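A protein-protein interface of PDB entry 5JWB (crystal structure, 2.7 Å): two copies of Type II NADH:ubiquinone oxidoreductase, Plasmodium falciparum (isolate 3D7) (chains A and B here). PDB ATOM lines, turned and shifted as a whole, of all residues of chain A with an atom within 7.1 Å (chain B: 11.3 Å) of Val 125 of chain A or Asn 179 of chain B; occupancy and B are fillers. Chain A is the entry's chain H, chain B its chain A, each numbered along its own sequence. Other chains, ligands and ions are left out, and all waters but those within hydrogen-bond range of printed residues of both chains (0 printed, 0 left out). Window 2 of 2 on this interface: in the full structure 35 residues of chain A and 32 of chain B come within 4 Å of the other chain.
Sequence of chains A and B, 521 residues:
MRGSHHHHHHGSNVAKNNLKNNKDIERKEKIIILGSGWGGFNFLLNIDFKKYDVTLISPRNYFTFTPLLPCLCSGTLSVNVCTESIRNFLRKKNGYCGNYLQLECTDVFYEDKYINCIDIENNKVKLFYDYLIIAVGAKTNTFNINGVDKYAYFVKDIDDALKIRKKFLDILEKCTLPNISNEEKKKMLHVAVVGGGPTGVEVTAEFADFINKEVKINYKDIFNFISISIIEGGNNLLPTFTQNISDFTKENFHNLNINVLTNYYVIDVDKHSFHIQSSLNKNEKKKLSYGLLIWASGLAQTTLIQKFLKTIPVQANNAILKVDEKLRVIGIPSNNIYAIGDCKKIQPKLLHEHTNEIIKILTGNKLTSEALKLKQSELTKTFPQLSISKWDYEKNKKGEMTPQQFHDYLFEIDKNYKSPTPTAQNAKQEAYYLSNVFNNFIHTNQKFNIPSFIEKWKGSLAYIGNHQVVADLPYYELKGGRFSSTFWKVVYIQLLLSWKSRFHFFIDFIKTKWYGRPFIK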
ATOM      1  N   LEU A 101      -3.526  13.804 -24.555  1.00  0.00           N
ATOM      2  CA  LEU A 101      -3.254  12.399 -24.815  1.00  0.00           C
ATOM      3  C   LEU A 101      -2.799  11.702 -23.528  1.00  0.00           C
ATOM      4  O   LEU A 101      -1.995  12.237 -22.770  1.00  0.00           O
ATOM      5  CB  LEU A 101      -2.197  12.245 -25.918  1.00  0.00           C
ATOM      6  CG  LEU A 101      -2.515  12.877 -27.288  1.00  0.00           C
ATOM      7  CD1 LEU A 101      -1.334  12.759 -28.260  1.00  0.00           C
ATOM      8  CD2 LEU A 101      -3.807  12.290 -27.889  1.00  0.00           C
ATOM      9  N   LEU A 103      -0.574   9.608 -22.196  1.00  0.00           N
ATOM     10  CA  LEU A 103       0.697   8.930 -22.396  1.00  0.00           C
ATOM     11  C   LEU A 103       1.686   9.332 -21.326  1.00  0.00           C
ATOM     12  O   LEU A 103       1.512  10.351 -20.667  1.00  0.00           O
ATOM     13  CB  LEU A 103       1.278   9.255 -23.769  1.00  0.00           C
ATOM     14  CG  LEU A 103       0.374   8.987 -24.963  1.00  0.00           C
ATOM     15  CD1 LEU A 103       0.921   9.696 -26.199  1.00  0.00           C
ATOM     16  CD2 LEU A 103       0.256   7.486 -25.171  1.00  0.00           C
ATOM     17  N   GLU A 104       2.721   8.514 -21.169  1.00  0.00           N
ATOM     18  CA  GLU A 104       3.866   8.840 -20.342  1.00  0.00           C
ATOM     19  C   GLU A 104       5.060   9.016 -21.254  1.00  0.00           C
ATOM     20  O   GLU A 104       5.436   8.087 -21.954  1.00  0.00           O
ATOM     21  CB  GLU A 104       4.132   7.744 -19.318  1.00  0.00           C
ATOM     22  CG  GLU A 104       5.555   7.728 -18.824  1.00  0.00           C
ATOM     23  CD  GLU A 104       5.883   6.507 -17.988  1.00  0.00           C
ATOM     24  OE1 GLU A 104       4.945   5.862 -17.473  1.00  0.00           O
ATOM     25  OE2 GLU A 104       7.086   6.190 -17.865  1.00  0.00           O
ATOM     26  N   THR A 106       8.831   9.082 -22.369  1.00  0.00           N
ATOM     27  CA  THR A 106       9.935   8.251 -21.882  1.00  0.00           C
ATOM     28  C   THR A 106      11.295   8.755 -22.345  1.00  0.00           C
ATOM     29  O   THR A 106      12.314   8.384 -21.768  1.00  0.00           O
ATOM     30  CB  THR A 106       9.794   6.779 -22.323  1.00  0.00           C
ATOM     31  OG1 THR A 106       9.625   6.717 -23.744  1.00  0.00           O
ATOM     32  CG2 THR A 106       8.605   6.111 -21.645  1.00  0.00           C
ATOM     33  N   TYR A 114      11.373  15.701 -31.290  1.00  0.00           N
ATOM     34  CA  TYR A 114      10.274  14.775 -31.048  1.00  0.00           C
ATOM     35  C   TYR A 114      10.432  14.132 -29.680  1.00  0.00           C
ATOM     36  O   TYR A 114      11.485  14.248 -29.051  1.00  0.00           O
ATOM     37  CB  TYR A 114      10.177  13.704 -32.155  1.00  0.00           C
ATOM     38  CG  TYR A 114      11.225  12.601 -32.138  1.00  0.00           C
ATOM     39  CD1 TYR A 114      12.393  12.709 -32.898  1.00  0.00           C
ATOM     40  CD2 TYR A 114      11.038  11.437 -31.396  1.00  0.00           C
ATOM     41  CE1 TYR A 114      13.360  11.693 -32.901  1.00  0.00           C
ATOM     42  CE2 TYR A 114      12.001  10.417 -31.392  1.00  0.00           C
ATOM     43  CZ  TYR A 114      13.161  10.554 -32.148  1.00  0.00           C
ATOM     44  OH  TYR A 114      14.127   9.564 -32.153  1.00  0.00           O
ATOM     45  N   ILE A 115       9.381  13.462 -29.215  1.00  0.00           N
ATOM     46  CA  ILE A 115       9.447  12.730 -27.955  1.00  0.00           C
ATOM     47  C   ILE A 115       8.887  11.329 -28.147  1.00  0.00           C
ATOM     48  O   ILE A 115       8.000  11.112 -28.963  1.00  0.00           O
ATOM     49  CB  ILE A 115       8.664  13.445 -26.819  1.00  0.00           C
ATOM     50  CG1 ILE A 115       7.203  13.672 -27.231  1.00  0.00           C
ATOM     51  CG2 ILE A 115       9.327  14.773 -26.436  1.00  0.00           C
ATOM     52  CD1 ILE A 115       6.249  13.886 -26.047  1.00  0.00           C
ATOM     53  N   ASN A 116       9.414  10.372 -27.400  1.00  0.00           N
ATOM     54  CA  ASN A 116       8.819   9.050 -27.362  1.00  0.00           C
ATOM     55  C   ASN A 116       7.913   8.904 -26.138  1.00  0.00           C
ATOM     56  O   ASN A 116       8.299   9.244 -25.011  1.00  0.00           O
ATOM     57  CB  ASN A 116       9.892   7.964 -27.330  1.00  0.00           C
ATOM     58  CG  ASN A 116      10.635   7.819 -28.642  1.00  0.00           C
ATOM     59  OD1 ASN A 116      10.222   8.347 -29.678  1.00  0.00           O
ATOM     60  ND2 ASN A 116      11.739   7.081 -28.606  1.00  0.00           N
ATOM     61  N   CYS A 117       6.715   8.381 -26.361  1.00  0.00           N
ATOM     62  CA  CYS A 117       5.819   8.078 -25.263  1.00  0.00           C
ATOM     63  C   CYS A 117       5.451   6.591 -25.261  1.00  0.00           C
ATOM     64  O   CYS A 117       5.789   5.863 -26.197  1.00  0.00           O
ATOM     65  CB  CYS A 117       4.571   8.949 -25.356  1.00  0.00           C
ATOM     66  SG  CYS A 117       4.904  10.721 -25.222  1.00  0.00           S
ATOM     67  N   ILE A 118       4.802   6.137 -24.191  1.00  0.00           N
ATOM     68  CA  ILE A 118       4.168   4.823 -24.167  1.00  0.00           C
ATOM     69  C   ILE A 118       2.764   4.973 -23.603  1.00  0.00           C
ATOM     70  O   ILE A 118       2.537   5.786 -22.704  1.00  0.00           O
ATOM     71  CB  ILE A 118       4.940   3.777 -23.320  1.00  0.00           C
ATOM     72  CG1 ILE A 118       5.183   4.290 -21.905  1.00  0.00           C
ATOM     73  CG2 ILE A 118       6.247   3.415 -23.968  1.00  0.00           C
ATOM     74  CD1 ILE A 118       5.887   3.299 -21.034  1.00  0.00           C
ATOM     75  N   ASP A 119       1.819   4.200 -24.129  1.00  0.00           N
ATOM     76  CA  ASP A 119       0.484   4.217 -23.572  1.00  0.00           C
ATOM     77  C   ASP A 119       0.484   3.272 -22.387  1.00  0.00           C
ATOM     78  O   ASP A 119       1.540   2.850 -21.934  1.00  0.00           O
ATOM     79  CB  ASP A 119      -0.576   3.845 -24.613  1.00  0.00           C
ATOM     80  CG  ASP A 119      -0.312   2.508 -25.298  1.00  0.00           C
ATOM     81  OD1 ASP A 119      -0.895   2.283 -26.382  1.00  0.00           O
ATOM     82  OD2 ASP A 119       0.458   1.680 -24.768  1.00  0.00           O
ATOM     83  N   ASN A 122       2.111  -0.191 -23.091  1.00  0.00           N
ATOM     84  CA  ASN A 122       3.521  -0.142 -23.490  1.00  0.00           C
ATOM     85  C   ASN A 122       3.759  -0.061 -24.989  1.00  0.00           C
ATOM     86  O   ASN A 122       4.831  -0.414 -25.474  1.00  0.00           O
ATOM     87  CB  ASN A 122       4.275  -1.339 -22.907  1.00  0.00           C
ATOM     88  CG  ASN A 122       4.758  -1.078 -21.497  1.00  0.00           C
ATOM     89  OD1 ASN A 122       5.910  -0.690 -21.289  1.00  0.00           O
ATOM     90  ND2 ASN A 122       3.871  -1.258 -20.521  1.00  0.00           N
ATOM     91  N   ASN A 123       2.760   0.421 -25.710  1.00  0.00           N
ATOM     92  CA  ASN A 123       2.920   0.725 -27.116  1.00  0.00           C
ATOM     93  C   ASN A 123       3.632   2.066 -27.278  1.00  0.00           C
ATOM     94  O   ASN A 123       3.202   3.059 -26.701  1.00  0.00           O
ATOM     95  CB  ASN A 123       1.557   0.764 -27.817  1.00  0.00           C
ATOM     96  CG  ASN A 123       0.821  -0.554 -27.743  1.00  0.00           C
ATOM     97  OD1 ASN A 123       1.383  -1.615 -28.031  1.00  0.00           O
ATOM     98  ND2 ASN A 123      -0.448  -0.497 -27.352  1.00  0.00           N
ATOM     99  N   LYS A 124       4.706   2.106 -28.062  1.00  0.00           N
ATOM    100  CA  LYS A 124       5.435   3.351 -28.295  1.00  0.00           C
ATOM    101  C   LYS A 124       4.632   4.303 -29.174  1.00  0.00           C
ATOM    102  O   LYS A 124       3.975   3.875 -30.118  1.00  0.00           O
ATOM    103  CB  LYS A 124       6.807   3.077 -28.936  1.00  0.00           C
ATOM    104  CG  LYS A 124       7.594   4.350 -29.312  1.00  0.00           C
ATOM    105  CD  LYS A 124       8.912   4.069 -30.057  1.00  0.00           C
ATOM    106  CE  LYS A 124       9.886   3.259 -29.198  1.00  0.00           C
ATOM    107  NZ  LYS A 124      11.161   2.931 -29.913  1.00  0.00           N
ATOM    108  N   VAL A 125       4.671   5.588 -28.829  1.00  0.00           N
ATOM    109  CA  VAL A 125       4.140   6.669 -29.651  1.00  0.00           C
ATOM    110  C   VAL A 125       5.246   7.721 -29.818  1.00  0.00           C
ATOM    111  O   VAL A 125       5.989   8.004 -28.873  1.00  0.00           O
ATOM    112  CB  VAL A 125       2.897   7.329 -29.021  1.00  0.00           C
ATOM    113  CG1 VAL A 125       2.366   8.440 -29.915  1.00  0.00           C
ATOM    114  CG2 VAL A 125       1.822   6.302 -28.742  1.00  0.00           C
ATOM    115  N   LYS A 126       5.356   8.292 -31.017  1.00  0.00           N
ATOM    116  CA  LYS A 126       6.373   9.277 -31.316  1.00  0.00           C
ATOM    117  C   LYS A 126       5.680  10.551 -31.784  1.00  0.00           C
ATOM    118  O   LYS A 126       4.793  10.488 -32.620  1.00  0.00           O
ATOM    119  CB  LYS A 126       7.338   8.728 -32.364  1.00  0.00           C
ATOM    120  CG  LYS A 126       8.067   9.773 -33.186  1.00  0.00           C
ATOM    121  CD  LYS A 126       9.255   9.163 -33.925  1.00  0.00           C
ATOM    122  CE  LYS A 126       9.974  10.187 -34.819  1.00  0.00           C
ATOM    123  NZ  LYS A 126      11.181   9.587 -35.474  1.00  0.00           N
ATOM    124  N   LEU A 127       6.057  11.699 -31.218  1.00  0.00           N
ATOM    125  CA  LEU A 127       5.334  12.951 -31.452  1.00  0.00           C
ATOM    126  C   LEU A 127       6.272  14.108 -31.711  1.00  0.00           C
ATOM    127  O   LEU A 127       7.316  14.230 -31.077  1.00  0.00           O
ATOM    128  CB  LEU A 127       4.426  13.292 -30.261  1.00  0.00           C
ATOM    129  CG  LEU A 127       3.257  12.316 -30.091  1.00  0.00           C
ATOM    130  CD1 LEU A 127       2.546  12.489 -28.782  1.00  0.00           C
ATOM    131  CD2 LEU A 127       2.294  12.504 -31.238  1.00  0.00           C
ATOM    132  N   ASP B 170     -11.362   4.408 -19.751  1.00  0.00           N
ATOM    133  CA  ASP B 170     -10.120   3.897 -20.305  1.00  0.00           C
ATOM    134  C   ASP B 170     -10.204   3.728 -21.805  1.00  0.00           C
ATOM    135  O   ASP B 170      -9.271   4.071 -22.510  1.00  0.00           O
ATOM    136  CB  ASP B 170      -9.755   2.563 -19.681  1.00  0.00           C
ATOM    137  CG  ASP B 170      -9.070   2.717 -18.350  1.00  0.00           C
ATOM    138  OD1 ASP B 170      -8.887   1.688 -17.651  1.00  0.00           O
ATOM    139  OD2 ASP B 170      -8.723   3.867 -18.002  1.00  0.00           O
ATOM    140  N   ILE B 171     -11.319   3.190 -22.296  1.00  0.00           N
ATOM    141  CA  ILE B 171     -11.424   2.890 -23.718  1.00  0.00           C
ATOM    142  C   ILE B 171     -11.464   4.179 -24.498  1.00  0.00           C
ATOM    143  O   ILE B 171     -10.817   4.292 -25.532  1.00  0.00           O
ATOM    144  CB  ILE B 171     -12.655   2.042 -24.063  1.00  0.00           C
ATOM    145  CG1 ILE B 171     -12.466   0.617 -23.550  1.00  0.00           C
ATOM    146  CG2 ILE B 171     -12.847   1.988 -25.577  1.00  0.00           C
ATOM    147  CD1 ILE B 171     -13.740  -0.183 -23.418  1.00  0.00           C
ATOM    148  N   LEU B 172     -12.206   5.155 -23.986  1.00  0.00           N
ATOM    149  CA  LEU B 172     -12.314   6.450 -24.642  1.00  0.00           C
ATOM    150  C   LEU B 172     -10.943   7.082 -24.852  1.00  0.00           C
ATOM    151  O   LEU B 172     -10.655   7.627 -25.920  1.00  0.00           O
ATOM    152  CB  LEU B 172     -13.199   7.391 -23.836  1.00  0.00           C
ATOM    153  CG  LEU B 172     -14.700   7.119 -23.855  1.00  0.00           C
ATOM    154  CD1 LEU B 172     -15.371   8.115 -22.950  1.00  0.00           C
ATOM    155  CD2 LEU B 172     -15.279   7.222 -25.262  1.00  0.00           C
ATOM    156  N   GLU B 173     -10.095   6.995 -23.833  1.00  0.00           N
ATOM    157  CA  GLU B 173      -8.770   7.572 -23.936  1.00  0.00           C
ATOM    158  C   GLU B 173      -7.893   6.756 -24.871  1.00  0.00           C
ATOM    159  O   GLU B 173      -7.094   7.320 -25.627  1.00  0.00           O
ATOM    160  CB  GLU B 173      -8.111   7.699 -22.562  1.00  0.00           C
ATOM    161  CG  GLU B 173      -8.726   8.773 -21.677  1.00  0.00           C
ATOM    162  CD  GLU B 173      -8.722  10.177 -22.303  1.00  0.00           C
ATOM    163  OE1 GLU B 173      -9.638  10.983 -21.995  1.00  0.00           O
ATOM    164  OE2 GLU B 173      -7.807  10.481 -23.102  1.00  0.00           O
ATOM    165  N   LYS B 174      -8.041   5.437 -24.836  1.00  0.00           N
ATOM    166  CA  LYS B 174      -7.220   4.595 -25.689  1.00  0.00           C
ATOM    167  C   LYS B 174      -7.534   4.872 -27.157  1.00  0.00           C
ATOM    168  O   LYS B 174      -6.669   4.728 -28.018  1.00  0.00           O
ATOM    169  CB  LYS B 174      -7.422   3.118 -25.358  1.00  0.00           C
ATOM    170  CG  LYS B 174      -6.515   2.181 -26.144  1.00  0.00           C
ATOM    171  CD  LYS B 174      -6.689   0.729 -25.705  1.00  0.00           C
ATOM    172  CE  LYS B 174      -6.059  -0.255 -26.699  1.00  0.00           C
ATOM    173  NZ  LYS B 174      -6.435  -1.674 -26.435  1.00  0.00           N
ATOM    174  N   CYS B 175      -8.761   5.307 -27.433  1.00  0.00           N
ATOM    175  CA  CYS B 175      -9.214   5.523 -28.794  1.00  0.00           C
ATOM    176  C   CYS B 175      -8.994   6.958 -29.247  1.00  0.00           C
ATOM    177  O   CYS B 175      -9.397   7.348 -30.339  1.00  0.00           O
ATOM    178  CB  CYS B 175     -10.696   5.159 -28.927  1.00  0.00           C
ATOM    179  SG  CYS B 175     -11.034   3.376 -28.915  1.00  0.00           S
ATOM    180  N   THR B 176      -8.358   7.757 -28.403  1.00  0.00           N
ATOM    181  CA  THR B 176      -8.031   9.126 -28.785  1.00  0.00           C
ATOM    182  C   THR B 176      -6.577   9.173 -29.242  1.00  0.00           C
ATOM    183  O   THR B 176      -6.185  10.072 -29.968  1.00  0.00           O
ATOM    184  CB  THR B 176      -8.307  10.092 -27.635  1.00  0.00           C
ATOM    185  OG1 THR B 176      -9.695   9.995 -27.292  1.00  0.00           O
ATOM    186  CG2 THR B 176      -8.001  11.524 -28.028  1.00  0.00           C
ATOM    187  N   LEU B 177      -5.806   8.157 -28.859  1.00  0.00           N
ATOM    188  CA  LEU B 177      -4.456   7.947 -29.375  1.00  0.00           C
ATOM    189  C   LEU B 177      -4.408   7.807 -30.905  1.00  0.00           C
ATOM    190  O   LEU B 177      -5.348   7.282 -31.515  1.00  0.00           O
ATOM    191  CB  LEU B 177      -3.852   6.706 -28.731  1.00  0.00           C
ATOM    192  CG  LEU B 177      -3.783   6.731 -27.213  1.00  0.00           C
ATOM    193  CD1 LEU B 177      -3.008   5.536 -26.694  1.00  0.00           C
ATOM    194  CD2 LEU B 177      -3.154   8.046 -26.759  1.00  0.00           C
ATOM    195  N   PRO B 178      -3.304   8.265 -31.535  1.00  0.00           N
ATOM    196  CA  PRO B 178      -3.095   8.180 -32.992  1.00  0.00           C
ATOM    197  C   PRO B 178      -2.649   6.799 -33.508  1.00  0.00           C
ATOM    198  O   PRO B 178      -2.869   6.487 -34.684  1.00  0.00           O
ATOM    199  CB  PRO B 178      -2.001   9.214 -33.237  1.00  0.00           C
ATOM    200  CG  PRO B 178      -1.217   9.230 -31.971  1.00  0.00           C
ATOM    201  CD  PRO B 178      -2.240   9.050 -30.877  1.00  0.00           C
ATOM    202  N   ASN B 179      -2.050   5.982 -32.645  1.00  0.00           N
ATOM    203  CA  ASN B 179      -1.635   4.622 -33.023  1.00  0.00           C
ATOM    204  C   ASN B 179      -2.790   3.627 -33.226  1.00  0.00           C
ATOM    205  O   ASN B 179      -2.614   2.420 -33.027  1.00  0.00           O
ATOM    206  CB  ASN B 179      -0.662   4.056 -31.967  1.00  0.00           C
ATOM    207  CG  ASN B 179      -1.235   4.082 -30.539  1.00  0.00           C
ATOM    208  OD1 ASN B 179      -1.273   5.128 -29.903  1.00  0.00           O
ATOM    209  ND2 ASN B 179      -1.647   2.924 -30.030  1.00  0.00           N
ATOM    210  N   ILE B 180      -3.961   4.137 -33.624  1.00  0.00           N
ATOM    211  CA  ILE B 180      -5.207   3.364 -33.664  1.00  0.00           C
ATOM    212  C   ILE B 180      -6.037   3.692 -34.904  1.00  0.00           C
ATOM    213  O   ILE B 180      -6.305   4.857 -35.191  1.00  0.00           O
ATOM    214  CB  ILE B 180      -6.095   3.630 -32.423  1.00  0.00           C
ATOM    215  CG1 ILE B 180      -5.293   3.561 -31.120  1.00  0.00           C
ATOM    216  CG2 ILE B 180      -7.246   2.644 -32.379  1.00  0.00           C
ATOM    217  CD1 ILE B 180      -4.938   2.154 -30.685  1.00  0.00           C
ATOM    218  N   SER B 181      -6.463   2.657 -35.623  1.00  0.00           N
ATOM    219  CA  SER B 181      -7.272   2.844 -36.823  1.00  0.00           C
ATOM    220  C   SER B 181      -8.749   3.045 -36.498  1.00  0.00           C
ATOM    221  O   SER B 181      -9.214   2.669 -35.426  1.00  0.00           O
ATOM    222  CB  SER B 181      -7.113   1.647 -37.762  1.00  0.00           C
ATOM    223  OG  SER B 181      -7.746   0.499 -37.225  1.00  0.00           O
ATOM    224  N   ASN B 182      -9.488   3.614 -37.442  1.00  0.00           N
ATOM    225  CA  ASN B 182     -10.922   3.800 -37.280  1.00  0.00           C
ATOM    226  C   ASN B 182     -11.709   2.498 -37.083  1.00  0.00           C
ATOM    227  O   ASN B 182     -12.739   2.499 -36.404  1.00  0.00           O
ATOM    228  CB  ASN B 182     -11.488   4.561 -38.474  1.00  0.00           C
ATOM    229  CG  ASN B 182     -11.164   6.047 -38.421  1.00  0.00           C
ATOM    230  OD1 ASN B 182     -10.290   6.482 -37.666  1.00  0.00           O
ATOM    231  ND2 ASN B 182     -11.866   6.831 -39.225  1.00  0.00           N
ATOM    232  N   GLU B 183     -11.242   1.387 -37.652  1.00  0.00           N
ATOM    233  CA  GLU B 183     -11.984   0.143 -37.482  1.00  0.00           C
ATOM    234  C   GLU B 183     -11.642  -0.504 -36.137  1.00  0.00           C
ATOM    235  O   GLU B 183     -12.490  -1.150 -35.528  1.00  0.00           O
ATOM    236  CB  GLU B 183     -11.730  -0.841 -38.629  1.00  0.00           C
ATOM    237  CG  GLU B 183     -12.703  -2.035 -38.596  1.00  0.00           C
ATOM    238  CD  GLU B 183     -12.211  -3.277 -39.345  1.00  0.00           C
ATOM    239  OE1 GLU B 183     -10.980  -3.436 -39.535  1.00  0.00           O
ATOM    240  OE2 GLU B 183     -13.067  -4.119 -39.710  1.00  0.00           O
ATOM    241  N   GLU B 184     -10.412  -0.326 -35.663  1.00  0.00           N
ATOM    242  CA  GLU B 184     -10.100  -0.715 -34.289  1.00  0.00           C
ATOM    243  C   GLU B 184     -11.009   0.074 -33.338  1.00  0.00           C
ATOM    244  O   GLU B 184     -11.553  -0.467 -32.378  1.00  0.00           O
ATOM    245  CB  GLU B 184      -8.626  -0.458 -33.943  1.00  0.00           C
ATOM    246  CG  GLU B 184      -7.600  -1.287 -34.716  1.00  0.00           C
ATOM    247  CD  GLU B 184      -6.154  -0.875 -34.393  1.00  0.00           C
ATOM    248  OE1 GLU B 184      -5.790  -0.815 -33.192  1.00  0.00           O
ATOM    249  OE2 GLU B 184      -5.384  -0.593 -35.339  1.00  0.00           O
ATOM    250  N   LYS B 185     -11.168   1.362 -33.618  1.00  0.00           N
ATOM    251  CA  LYS B 185     -11.978   2.212 -32.764  1.00  0.00           C
ATOM    252  C   LYS B 185     -13.418   1.725 -32.718  1.00  0.00           C
ATOM    253  O   LYS B 185     -13.990   1.618 -31.640  1.00  0.00           O
ATOM    254  CB  LYS B 185     -11.920   3.664 -33.231  1.00  0.00           C
ATOM    255  CG  LYS B 185     -10.587   4.339 -32.970  1.00  0.00           C
ATOM    256  CD  LYS B 185     -10.584   5.771 -33.505  1.00  0.00           C
ATOM    257  CE  LYS B 185      -9.196   6.399 -33.379  1.00  0.00           C
ATOM    258  NZ  LYS B 185      -9.211   7.810 -33.852  1.00  0.00           N
ATOM    259  N   MET B 188     -13.693  -1.410 -30.558  1.00  0.00           N
ATOM    260  CA  MET B 188     -13.442  -1.166 -29.140  1.00  0.00           C
ATOM    261  C   MET B 188     -14.501  -0.284 -28.476  1.00  0.00           C
ATOM    262  O   MET B 188     -14.689  -0.351 -27.268  1.00  0.00           O
ATOM    263  CB  MET B 188     -12.061  -0.527 -28.949  1.00  0.00           C
ATOM    264  CG  MET B 188     -10.888  -1.462 -29.216  1.00  0.00           C
ATOM    265  SD  MET B 188      -9.295  -0.733 -28.748  1.00  0.00           S
ATOM    266  CE  MET B 188      -9.123   0.560 -29.976  1.00  0.00           C
ATOM    267  N   ILE B 222     -14.312  11.013 -31.935  1.00  0.00           N
ATOM    268  CA  ILE B 222     -14.565   9.579 -31.935  1.00  0.00           C
ATOM    269  C   ILE B 222     -15.999   9.205 -31.552  1.00  0.00           C
ATOM    270  O   ILE B 222     -16.340   8.022 -31.531  1.00  0.00           O
ATOM    271  CB  ILE B 222     -13.620   8.834 -30.996  1.00  0.00           C
ATOM    272  CG1 ILE B 222     -13.900   9.204 -29.546  1.00  0.00           C
ATOM    273  CG2 ILE B 222     -12.183   9.101 -31.359  1.00  0.00           C
ATOM    274  CD1 ILE B 222     -13.043   8.436 -28.561  1.00  0.00           C
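No position is printed for both chains.
CD2 of Leu 101 of chain A touches O of Thr 176 of chain B (3.9 Å).
Leu 103 of chain A touches Leu 177 of chain B (CD2 to CD2, 3.8 Å).
Asp 119 of chain A touches Leu 177 of chain B (CB to CD1, 3.6 Å).
OD1 of Asp 119 of chain A touches ND2 of Asn 179 of chain B, at 3.8 Å.
Asn 179 of chain B touches Val 125 of chain A.
N of Cys 117 of chain A is in hydrogen-bond range of O of Val 125 of chain A, 2.6 Å away.
The backbone carbonyl oxygen of Leu 172 of chain B lies within hydrogen-bond range of the side-chain hydroxyl of Thr 176 of chain B.
N of Asn 122 of chain A is in hydrogen-bond range of OD2 of Asp 119 of chain A (3.0 Å).
The backbone NH (N) of Asn 123 of chain A lies within hydrogen-bond range of the side-chain carboxylate (OD2) of Asp 119 of chain A, at 2.8 Å.
Of the 16 printed residues of chain A, 4 touch a printed residue of chain B.
Along chain A the printed residues that touch a printed residue of chain B span positions 101 to 125.
Of the 18 printed residues of chain B, 3 touch a printed residue of chain A.
Printed residues of chain B that touch a printed residue of chain A: Thr 176, Leu 177 and Asn 179.
Hydrophobic or aromatic side chains of chain B that line the printed part of chain A: Leu 177.
Printed residues of chain B within 4 Å of Leu 103 of chain A: Leu 177 (3.8 Å).
Ile 115 of chain A touches none of the printed residues of chain B.
No residue of chain B comes within 4 Å of Asn 116 of chain A.
No residue of chain B comes within 4 Å of Cys 117 of chain A.
Of the printed residues of chain B, Asp 119 of chain A touches Leu 177 (3.6 Å) and Asn 179 (3.8 Å).
Val 125 of chain A touches one residue of chain B.
No residue of chain B comes within 4 Å of Leu 127 of chain A.
Of the printed residues of chain A, Asn 179 of chain B touches Asp 119 and Val 125.
The nearest residue of chain B that does not touch Val 125 of chain A is Pro 178 of chain B (4.2 Å).
The nearest residue of chain A that does not touch Asn 179 of chain B is Asn 123 of chain A (4.5 Å).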
